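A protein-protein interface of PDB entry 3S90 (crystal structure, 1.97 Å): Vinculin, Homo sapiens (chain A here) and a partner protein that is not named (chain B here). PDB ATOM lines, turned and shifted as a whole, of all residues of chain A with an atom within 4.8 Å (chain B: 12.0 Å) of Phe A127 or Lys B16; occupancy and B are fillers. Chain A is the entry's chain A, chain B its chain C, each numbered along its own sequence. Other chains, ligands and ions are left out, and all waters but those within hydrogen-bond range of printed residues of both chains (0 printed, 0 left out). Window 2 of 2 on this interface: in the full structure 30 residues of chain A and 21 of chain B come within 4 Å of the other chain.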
ATOM      1  N   THR A  62     -18.223 -16.116  -8.214  1.00  0.00           N
ATOM      2  CA  THR A  62     -19.416 -16.949  -8.164  1.00  0.00           C
ATOM      3  C   THR A  62     -19.247 -17.981  -7.044  1.00  0.00           C
ATOM      4  O   THR A  62     -20.144 -18.086  -6.218  1.00  0.00           O
ATOM      5  CB  THR A  62     -19.703 -17.601  -9.533  1.00  0.00           C
ATOM      6  OG1 THR A  62     -19.678 -16.602 -10.553  1.00  0.00           O
ATOM      7  CG2 THR A  62     -21.032 -18.334  -9.554  1.00  0.00           C
ATOM      8  N   LEU A  71     -21.274 -26.688  -6.970  1.00  0.00           N
ATOM      9  CA  LEU A  71     -20.611 -25.668  -7.801  1.00  0.00           C
ATOM     10  C   LEU A  71     -19.265 -25.263  -7.155  1.00  0.00           C
ATOM     11  O   LEU A  71     -18.256 -25.168  -7.852  1.00  0.00           O
ATOM     12  CB  LEU A  71     -21.515 -24.425  -8.034  1.00  0.00           C
ATOM     13  CG  LEU A  71     -20.908 -23.316  -8.935  1.00  0.00           C
ATOM     14  CD1 LEU A  71     -21.944 -22.602  -9.719  1.00  0.00           C
ATOM     15  CD2 LEU A  71     -20.114 -22.293  -8.126  1.00  0.00           C
ATOM     16  N   MET A  75     -16.060 -26.145  -9.692  1.00  0.00           N
ATOM     17  CA  MET A  75     -15.441 -25.059 -10.472  1.00  0.00           C
ATOM     18  C   MET A  75     -13.892 -25.033 -10.348  1.00  0.00           C
ATOM     19  O   MET A  75     -13.229 -24.896 -11.377  1.00  0.00           O
ATOM     20  CB  MET A  75     -16.021 -23.697 -10.093  1.00  0.00           C
ATOM     21  CG  MET A  75     -17.417 -23.497 -10.613  1.00  0.00           C
ATOM     22  SD  MET A  75     -17.700 -21.804 -11.135  1.00  0.00           S
ATOM     23  CE  MET A  75     -18.857 -22.109 -12.460  1.00  0.00           C
ATOM     24  N   LEU A 123     -16.950 -25.496 -16.935  1.00  0.00           N
ATOM     25  CA  LEU A 123     -17.413 -24.319 -16.187  1.00  0.00           C
ATOM     26  C   LEU A 123     -18.844 -23.936 -16.555  1.00  0.00           C
ATOM     27  O   LEU A 123     -19.636 -23.675 -15.659  1.00  0.00           O
ATOM     28  CB  LEU A 123     -16.478 -23.119 -16.397  1.00  0.00           C
ATOM     29  CG  LEU A 123     -15.175 -23.171 -15.624  1.00  0.00           C
ATOM     30  CD1 LEU A 123     -14.222 -22.113 -16.089  1.00  0.00           C
ATOM     31  CD2 LEU A 123     -15.413 -23.067 -14.130  1.00  0.00           C
ATOM     32  N   LEU A 124     -19.181 -23.921 -17.858  1.00  0.00           N
ATOM     33  CA  LEU A 124     -20.539 -23.584 -18.312  1.00  0.00           C
ATOM     34  C   LEU A 124     -21.542 -24.650 -17.889  1.00  0.00           C
ATOM     35  O   LEU A 124     -22.632 -24.300 -17.424  1.00  0.00           O
ATOM     36  CB  LEU A 124     -20.585 -23.376 -19.828  1.00  0.00           C
ATOM     37  CG  LEU A 124     -19.946 -22.087 -20.344  1.00  0.00           C
ATOM     38  CD1 LEU A 124     -19.727 -22.167 -21.858  1.00  0.00           C
ATOM     39  CD2 LEU A 124     -20.756 -20.842 -19.933  1.00  0.00           C
ATOM     40  N   LEU A 125     -21.165 -25.942 -17.991  1.00  0.00           N
ATOM     41  CA  LEU A 125     -22.054 -27.040 -17.586  1.00  0.00           C
ATOM     42  C   LEU A 125     -22.277 -27.032 -16.056  1.00  0.00           C
ATOM     43  O   LEU A 125     -23.411 -27.218 -15.605  1.00  0.00           O
ATOM     44  CB  LEU A 125     -21.519 -28.397 -18.079  1.00  0.00           C
ATOM     45  CG  LEU A 125     -21.697 -28.646 -19.596  1.00  0.00           C
ATOM     46  CD1 LEU A 125     -20.732 -29.731 -20.123  1.00  0.00           C
ATOM     47  CD2 LEU A 125     -23.115 -29.038 -19.932  1.00  0.00           C
ATOM     48  N   THR A 126     -21.216 -26.760 -15.265  1.00  0.00           N
ATOM     49  CA  THR A 126     -21.334 -26.671 -13.809  1.00  0.00           C
ATOM     50  C   THR A 126     -22.249 -25.516 -13.428  1.00  0.00           C
ATOM     51  O   THR A 126     -23.100 -25.686 -12.554  1.00  0.00           O
ATOM     52  CB  THR A 126     -19.945 -26.519 -13.160  1.00  0.00           C
ATOM     53  OG1 THR A 126     -19.204 -27.709 -13.429  1.00  0.00           O
ATOM     54  CG2 THR A 126     -20.014 -26.278 -11.646  1.00  0.00           C
ATOM     55  N   PHE A 127     -22.064 -24.345 -14.063  1.00  0.00           N
ATOM     56  CA  PHE A 127     -22.869 -23.160 -13.785  1.00  0.00           C
ATOM     57  C   PHE A 127     -24.332 -23.423 -14.129  1.00  0.00           C
ATOM     58  O   PHE A 127     -25.216 -23.069 -13.346  1.00  0.00           O
ATOM     59  CB  PHE A 127     -22.331 -21.945 -14.549  1.00  0.00           C
ATOM     60  CG  PHE A 127     -22.909 -20.631 -14.090  1.00  0.00           C
ATOM     61  CD1 PHE A 127     -22.306 -19.906 -13.070  1.00  0.00           C
ATOM     62  CD2 PHE A 127     -24.057 -20.111 -14.683  1.00  0.00           C
ATOM     63  CE1 PHE A 127     -22.840 -18.685 -12.650  1.00  0.00           C
ATOM     64  CE2 PHE A 127     -24.609 -18.902 -14.242  1.00  0.00           C
ATOM     65  CZ  PHE A 127     -23.997 -18.198 -13.229  1.00  0.00           C
ATOM     66  N   ASP A 128     -24.579 -24.091 -15.264  1.00  0.00           N
ATOM     67  CA  ASP A 128     -25.930 -24.427 -15.706  1.00  0.00           C
ATOM     68  C   ASP A 128     -26.613 -25.410 -14.746  1.00  0.00           C
ATOM     69  O   ASP A 128     -27.795 -25.242 -14.457  1.00  0.00           O
ATOM     70  CB  ASP A 128     -25.930 -24.993 -17.132  1.00  0.00           C
ATOM     71  CG  ASP A 128     -27.338 -25.075 -17.692  1.00  0.00           C
ATOM     72  OD1 ASP A 128     -27.907 -24.014 -18.013  1.00  0.00           O
ATOM     73  OD2 ASP A 128     -27.906 -26.185 -17.703  1.00  0.00           O
ATOM     74  N   GLU A 129     -25.881 -26.441 -14.281  1.00  0.00           N
ATOM     75  CA  GLU A 129     -26.425 -27.439 -13.366  1.00  0.00           C
ATOM     76  C   GLU A 129     -26.824 -26.793 -12.022  1.00  0.00           C
ATOM     77  O   GLU A 129     -27.870 -27.145 -11.476  1.00  0.00           O
ATOM     78  CB  GLU A 129     -25.443 -28.589 -13.153  1.00  0.00           C
ATOM     79  CG  GLU A 129     -25.402 -29.549 -14.333  1.00  0.00           C
ATOM     80  CD  GLU A 129     -24.241 -30.527 -14.370  1.00  0.00           C
ATOM     81  OE1 GLU A 129     -23.627 -30.781 -13.307  1.00  0.00           O
ATOM     82  OE2 GLU A 129     -23.966 -31.068 -15.466  1.00  0.00           O
ATOM     83  N   ALA A 130     -26.051 -25.796 -11.555  1.00  0.00           N
ATOM     84  CA  ALA A 130     -26.362 -25.048 -10.329  1.00  0.00           C
ATOM     85  C   ALA A 130     -27.647 -24.195 -10.528  1.00  0.00           C
ATOM     86  O   ALA A 130     -28.466 -24.123  -9.615  1.00  0.00           O
ATOM     87  CB  ALA A 130     -25.189 -24.168  -9.935  1.00  0.00           C
ATOM     88  N   GLU A 131     -27.838 -23.596 -11.727  1.00  0.00           N
ATOM     89  CA  GLU A 131     -29.041 -22.802 -12.020  1.00  0.00           C
ATOM     90  C   GLU A 131     -30.273 -23.709 -12.026  1.00  0.00           C
ATOM     91  O   GLU A 131     -31.329 -23.337 -11.507  1.00  0.00           O
ATOM     92  CB  GLU A 131     -28.908 -22.045 -13.352  1.00  0.00           C
ATOM     93  CG  GLU A 131     -27.964 -20.851 -13.300  1.00  0.00           C
ATOM     94  CD  GLU A 131     -28.328 -19.739 -12.330  1.00  0.00           C
ATOM     95  OE1 GLU A 131     -29.513 -19.336 -12.298  1.00  0.00           O
ATOM     96  OE2 GLU A 131     -27.420 -19.261 -11.611  1.00  0.00           O
ATOM     97  N   GLU A 182     -34.656 -21.506 -23.033  1.00  0.00           N
ATOM     98  CA  GLU A 182     -33.205 -21.667 -23.146  1.00  0.00           C
ATOM     99  C   GLU A 182     -32.820 -23.032 -23.740  1.00  0.00           C
ATOM    100  O   GLU A 182     -31.688 -23.194 -24.192  1.00  0.00           O
ATOM    101  CB  GLU A 182     -32.553 -21.513 -21.757  1.00  0.00           C
ATOM    102  CG  GLU A 182     -32.611 -20.101 -21.180  1.00  0.00           C
ATOM    103  CD  GLU A 182     -32.332 -19.922 -19.690  1.00  0.00           C
ATOM    104  OE1 GLU A 182     -32.731 -18.863 -19.150  1.00  0.00           O
ATOM    105  OE2 GLU A 182     -31.719 -20.820 -19.063  1.00  0.00           O
ATOM    106  N   THR B  14     -25.391  -8.385 -14.039  1.00  0.00           N
ATOM    107  CA  THR B  14     -25.524  -9.419 -13.011  1.00  0.00           C
ATOM    108  C   THR B  14     -24.339 -10.405 -13.074  1.00  0.00           C
ATOM    109  O   THR B  14     -23.572 -10.392 -14.041  1.00  0.00           O
ATOM    110  CB  THR B  14     -26.898 -10.133 -13.105  1.00  0.00           C
ATOM    111  OG1 THR B  14     -26.992 -11.119 -12.074  1.00  0.00           O
ATOM    112  CG2 THR B  14     -27.160 -10.782 -14.468  1.00  0.00           C
ATOM    113  N   ALA B  15     -24.199 -11.249 -12.029  1.00  0.00           N
ATOM    114  CA  ALA B  15     -23.143 -12.258 -11.884  1.00  0.00           C
ATOM    115  C   ALA B  15     -23.215 -13.337 -12.978  1.00  0.00           C
ATOM    116  O   ALA B  15     -22.167 -13.803 -13.439  1.00  0.00           O
ATOM    117  CB  ALA B  15     -23.224 -12.906 -10.510  1.00  0.00           C
ATOM    118  N   LYS B  16     -24.447 -13.721 -13.390  1.00  0.00           N
ATOM    119  CA  LYS B  16     -24.701 -14.705 -14.446  1.00  0.00           C
ATOM    120  C   LYS B  16     -24.228 -14.145 -15.794  1.00  0.00           C
ATOM    121  O   LYS B  16     -23.493 -14.831 -16.513  1.00  0.00           O
ATOM    122  CB  LYS B  16     -26.198 -15.081 -14.491  1.00  0.00           C
ATOM    123  CG  LYS B  16     -26.559 -16.135 -15.542  1.00  0.00           C
ATOM    124  CD  LYS B  16     -28.062 -16.361 -15.637  1.00  0.00           C
ATOM    125  CE  LYS B  16     -28.412 -17.371 -16.703  1.00  0.00           C
ATOM    126  NZ  LYS B  16     -29.883 -17.549 -16.832  1.00  0.00           N
ATOM    127  N   ARG B  17     -24.623 -12.887 -16.111  1.00  0.00           N
ATOM    128  CA  ARG B  17     -24.265 -12.193 -17.352  1.00  0.00           C
ATOM    129  C   ARG B  17     -22.751 -11.976 -17.440  1.00  0.00           C
ATOM    130  O   ARG B  17     -22.188 -12.158 -18.516  1.00  0.00           O
ATOM    131  CB  ARG B  17     -25.012 -10.863 -17.473  1.00  0.00           C
ATOM    132  CG  ARG B  17     -25.220 -10.420 -18.919  1.00  0.00           C
ATOM    133  CD  ARG B  17     -26.339  -9.416 -19.029  1.00  0.00           C
ATOM    134  NE  ARG B  17     -27.661 -10.002 -18.779  1.00  0.00           N
ATOM    135  CZ  ARG B  17     -28.811  -9.337 -18.838  1.00  0.00           C
ATOM    136  NH1 ARG B  17     -28.826  -8.047 -19.158  1.00  0.00           N
ATOM    137  NH2 ARG B  17     -29.956  -9.957 -18.589  1.00  0.00           N
ATOM    138  N   GLN B  18     -22.102 -11.627 -16.306  1.00  0.00           N
ATOM    139  CA  GLN B  18     -20.661 -11.397 -16.204  1.00  0.00           C
ATOM    140  C   GLN B  18     -19.890 -12.700 -16.456  1.00  0.00           C
ATOM    141  O   GLN B  18     -18.908 -12.685 -17.197  1.00  0.00           O
ATOM    142  CB  GLN B  18     -20.312 -10.820 -14.826  1.00  0.00           C
ATOM    143  CG  GLN B  18     -19.082  -9.921 -14.819  1.00  0.00           C
ATOM    144  CD  GLN B  18     -18.784  -9.347 -13.454  1.00  0.00           C
ATOM    145  OE1 GLN B  18     -19.677  -8.910 -12.712  1.00  0.00           O
ATOM    146  NE2 GLN B  18     -17.507  -9.289 -13.112  1.00  0.00           N
ATOM    147  N   PHE B  19     -20.358 -13.825 -15.862  1.00  0.00           N
ATOM    148  CA  PHE B  19     -19.758 -15.151 -16.020  1.00  0.00           C
ATOM    149  C   PHE B  19     -19.847 -15.622 -17.468  1.00  0.00           C
ATOM    150  O   PHE B  19     -18.840 -16.070 -18.022  1.00  0.00           O
ATOM    151  CB  PHE B  19     -20.418 -16.179 -15.079  1.00  0.00           C
ATOM    152  CG  PHE B  19     -19.840 -17.572 -15.203  1.00  0.00           C
ATOM    153  CD1 PHE B  19     -18.693 -17.931 -14.505  1.00  0.00           C
ATOM    154  CD2 PHE B  19     -20.425 -18.511 -16.045  1.00  0.00           C
ATOM    155  CE1 PHE B  19     -18.145 -19.209 -14.644  1.00  0.00           C
ATOM    156  CE2 PHE B  19     -19.870 -19.786 -16.188  1.00  0.00           C
ATOM    157  CZ  PHE B  19     -18.737 -20.127 -15.486  1.00  0.00           C
ATOM    158  N   VAL B  20     -21.053 -15.539 -18.063  1.00  0.00           N
ATOM    159  CA  VAL B  20     -21.343 -15.957 -19.435  1.00  0.00           C
ATOM    160  C   VAL B  20     -20.507 -15.119 -20.419  1.00  0.00           C
ATOM    161  O   VAL B  20     -19.874 -15.705 -21.299  1.00  0.00           O
ATOM    162  CB  VAL B  20     -22.867 -15.910 -19.726  1.00  0.00           C
ATOM    163  CG1 VAL B  20     -23.172 -15.898 -21.221  1.00  0.00           C
ATOM    164  CG2 VAL B  20     -23.582 -17.071 -19.046  1.00  0.00           C
ATOM    165  N   GLN B  21     -20.455 -13.777 -20.232  1.00  0.00           N
ATOM    166  CA  GLN B  21     -19.663 -12.859 -21.069  1.00  0.00           C
ATOM    167  C   GLN B  21     -18.161 -13.204 -21.004  1.00  0.00           C
ATOM    168  O   GLN B  21     -17.475 -13.115 -22.025  1.00  0.00           O
ATOM    169  CB  GLN B  21     -19.905 -11.387 -20.661  1.00  0.00           C
ATOM    170  CG  GLN B  21     -19.297 -10.329 -21.607  1.00  0.00           C
ATOM    171  CD  GLN B  21     -19.666 -10.512 -23.065  1.00  0.00           C
ATOM    172  OE1 GLN B  21     -20.844 -10.538 -23.442  1.00  0.00           O
ATOM    173  NE2 GLN B  21     -18.657 -10.648 -23.920  1.00  0.00           N
ATOM    174  N   SER B  22     -17.666 -13.603 -19.812  1.00  0.00           N
ATOM    175  CA  SER B  22     -16.279 -14.018 -19.593  1.00  0.00           C
ATOM    176  C   SER B  22     -15.963 -15.291 -20.387  1.00  0.00           C
ATOM    177  O   SER B  22     -14.913 -15.349 -21.027  1.00  0.00           O
ATOM    178  CB  SER B  22     -16.008 -14.241 -18.110  1.00  0.00           C
ATOM    179  OG  SER B  22     -15.919 -12.993 -17.449  1.00  0.00           O
ATOM    180  N   ALA B  23     -16.881 -16.289 -20.367  1.00  0.00           N
ATOM    181  CA  ALA B  23     -16.748 -17.553 -21.096  1.00  0.00           C
ATOM    182  C   ALA B  23     -16.750 -17.295 -22.591  1.00  0.00           C
ATOM    183  O   ALA B  23     -15.914 -17.856 -23.304  1.00  0.00           O
ATOM    184  CB  ALA B  23     -17.869 -18.502 -20.725  1.00  0.00           C
ATOM    185  N   LYS B  24     -17.662 -16.411 -23.059  1.00  0.00           N
ATOM    186  CA  LYS B  24     -17.773 -16.005 -24.462  1.00  0.00           C
ATOM    187  C   LYS B  24     -16.447 -15.406 -24.950  1.00  0.00           C
ATOM    188  O   LYS B  24     -16.011 -15.738 -26.048  1.00  0.00           O
ATOM    189  CB  LYS B  24     -18.918 -14.994 -24.633  1.00  0.00           C
ATOM    190  CG  LYS B  24     -19.693 -15.160 -25.924  1.00  0.00           C
ATOM    191  CD  LYS B  24     -20.871 -14.188 -25.986  1.00  0.00           C
ATOM    192  CE  LYS B  24     -21.813 -14.461 -27.139  1.00  0.00           C
ATOM    193  NZ  LYS B  24     -21.229 -14.071 -28.450  1.00  0.00           N
ATOM    194  N   GLU B  25     -15.784 -14.581 -24.104  1.00  0.00           N
ATOM    195  CA  GLU B  25     -14.504 -13.936 -24.409  1.00  0.00           C
ATOM    196  C   GLU B  25     -13.374 -14.963 -24.594  1.00  0.00           C
ATOM    197  O   GLU B  25     -12.544 -14.801 -25.493  1.00  0.00           O
ATOM    198  CB  GLU B  25     -14.128 -12.928 -23.314  1.00  0.00           C
ATOM    199  CG  GLU B  25     -13.454 -11.681 -23.860  1.00  0.00           C
ATOM    200  CD  GLU B  25     -14.398 -10.710 -24.547  1.00  0.00           C
ATOM    201  OE1 GLU B  25     -14.992  -9.862 -23.843  1.00  0.00           O
ATOM    202  OE2 GLU B  25     -14.568 -10.815 -25.784  1.00  0.00           O
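Of the 13 printed residues of chain A, 5 touch a printed residue of chain B.
Printed residues of chain A that touch a printed residue of chain B: Met A75, Leu A123, Leu A124, Phe A127 and Glu A182.
Hydrophobic or aromatic side chains of chain A within 4 Å of the printed part of chain B: Met A75, Leu A123, Leu A124 and Phe A127.
Of the 12 printed residues of chain B, 3 touch a printed residue of chain A.
Met A75 touches Phe B19 (CE to CZ, 3.6 Å).
O of Leu A123 touches CZ of Phe B19, at 3.7 Å.
CE2 of Phe B19 touches CD2 of Leu A124, at 3.99 Å.
Ala B23 touches Leu A124.
Lys B16 touches Phe A127.
Phe A127 touches Phe B19 (CB to CE2, 3.7 Å).
NZ of Lys B16 lies within salt-bridge range of OE1 of Glu A182.
Of the printed residues of chain B, Phe A127 touches Lys B16 (3.6 Å) and Phe B19 (3.7 Å).
No residue of chain B comes within 4 Å of Thr A126.
No residue of chain B comes within 4 Å of Asp A128.
Ala A130 touches none of the printed residues of chain B.
Of the printed residues of chain A, Ala B23 touches Leu A124.
Of the printed residues of chain B, Met A75 touches Phe B19.
Printed residues of chain B within 4 Å of Leu A124: Phe B19 and Ala B23.
Printed residues of chain A within 4 Å of Phe B19: Met A75 (3.6 Å), Leu A123 (3.7 Å), Leu A124 (3.99 Å) and Phe A127 (3.7 Å).
Leu A125 touches none of the printed residues of chain B.
The nearest residue of chain B that does not touch Phe A127 is Ala B15 (4.8 Å).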
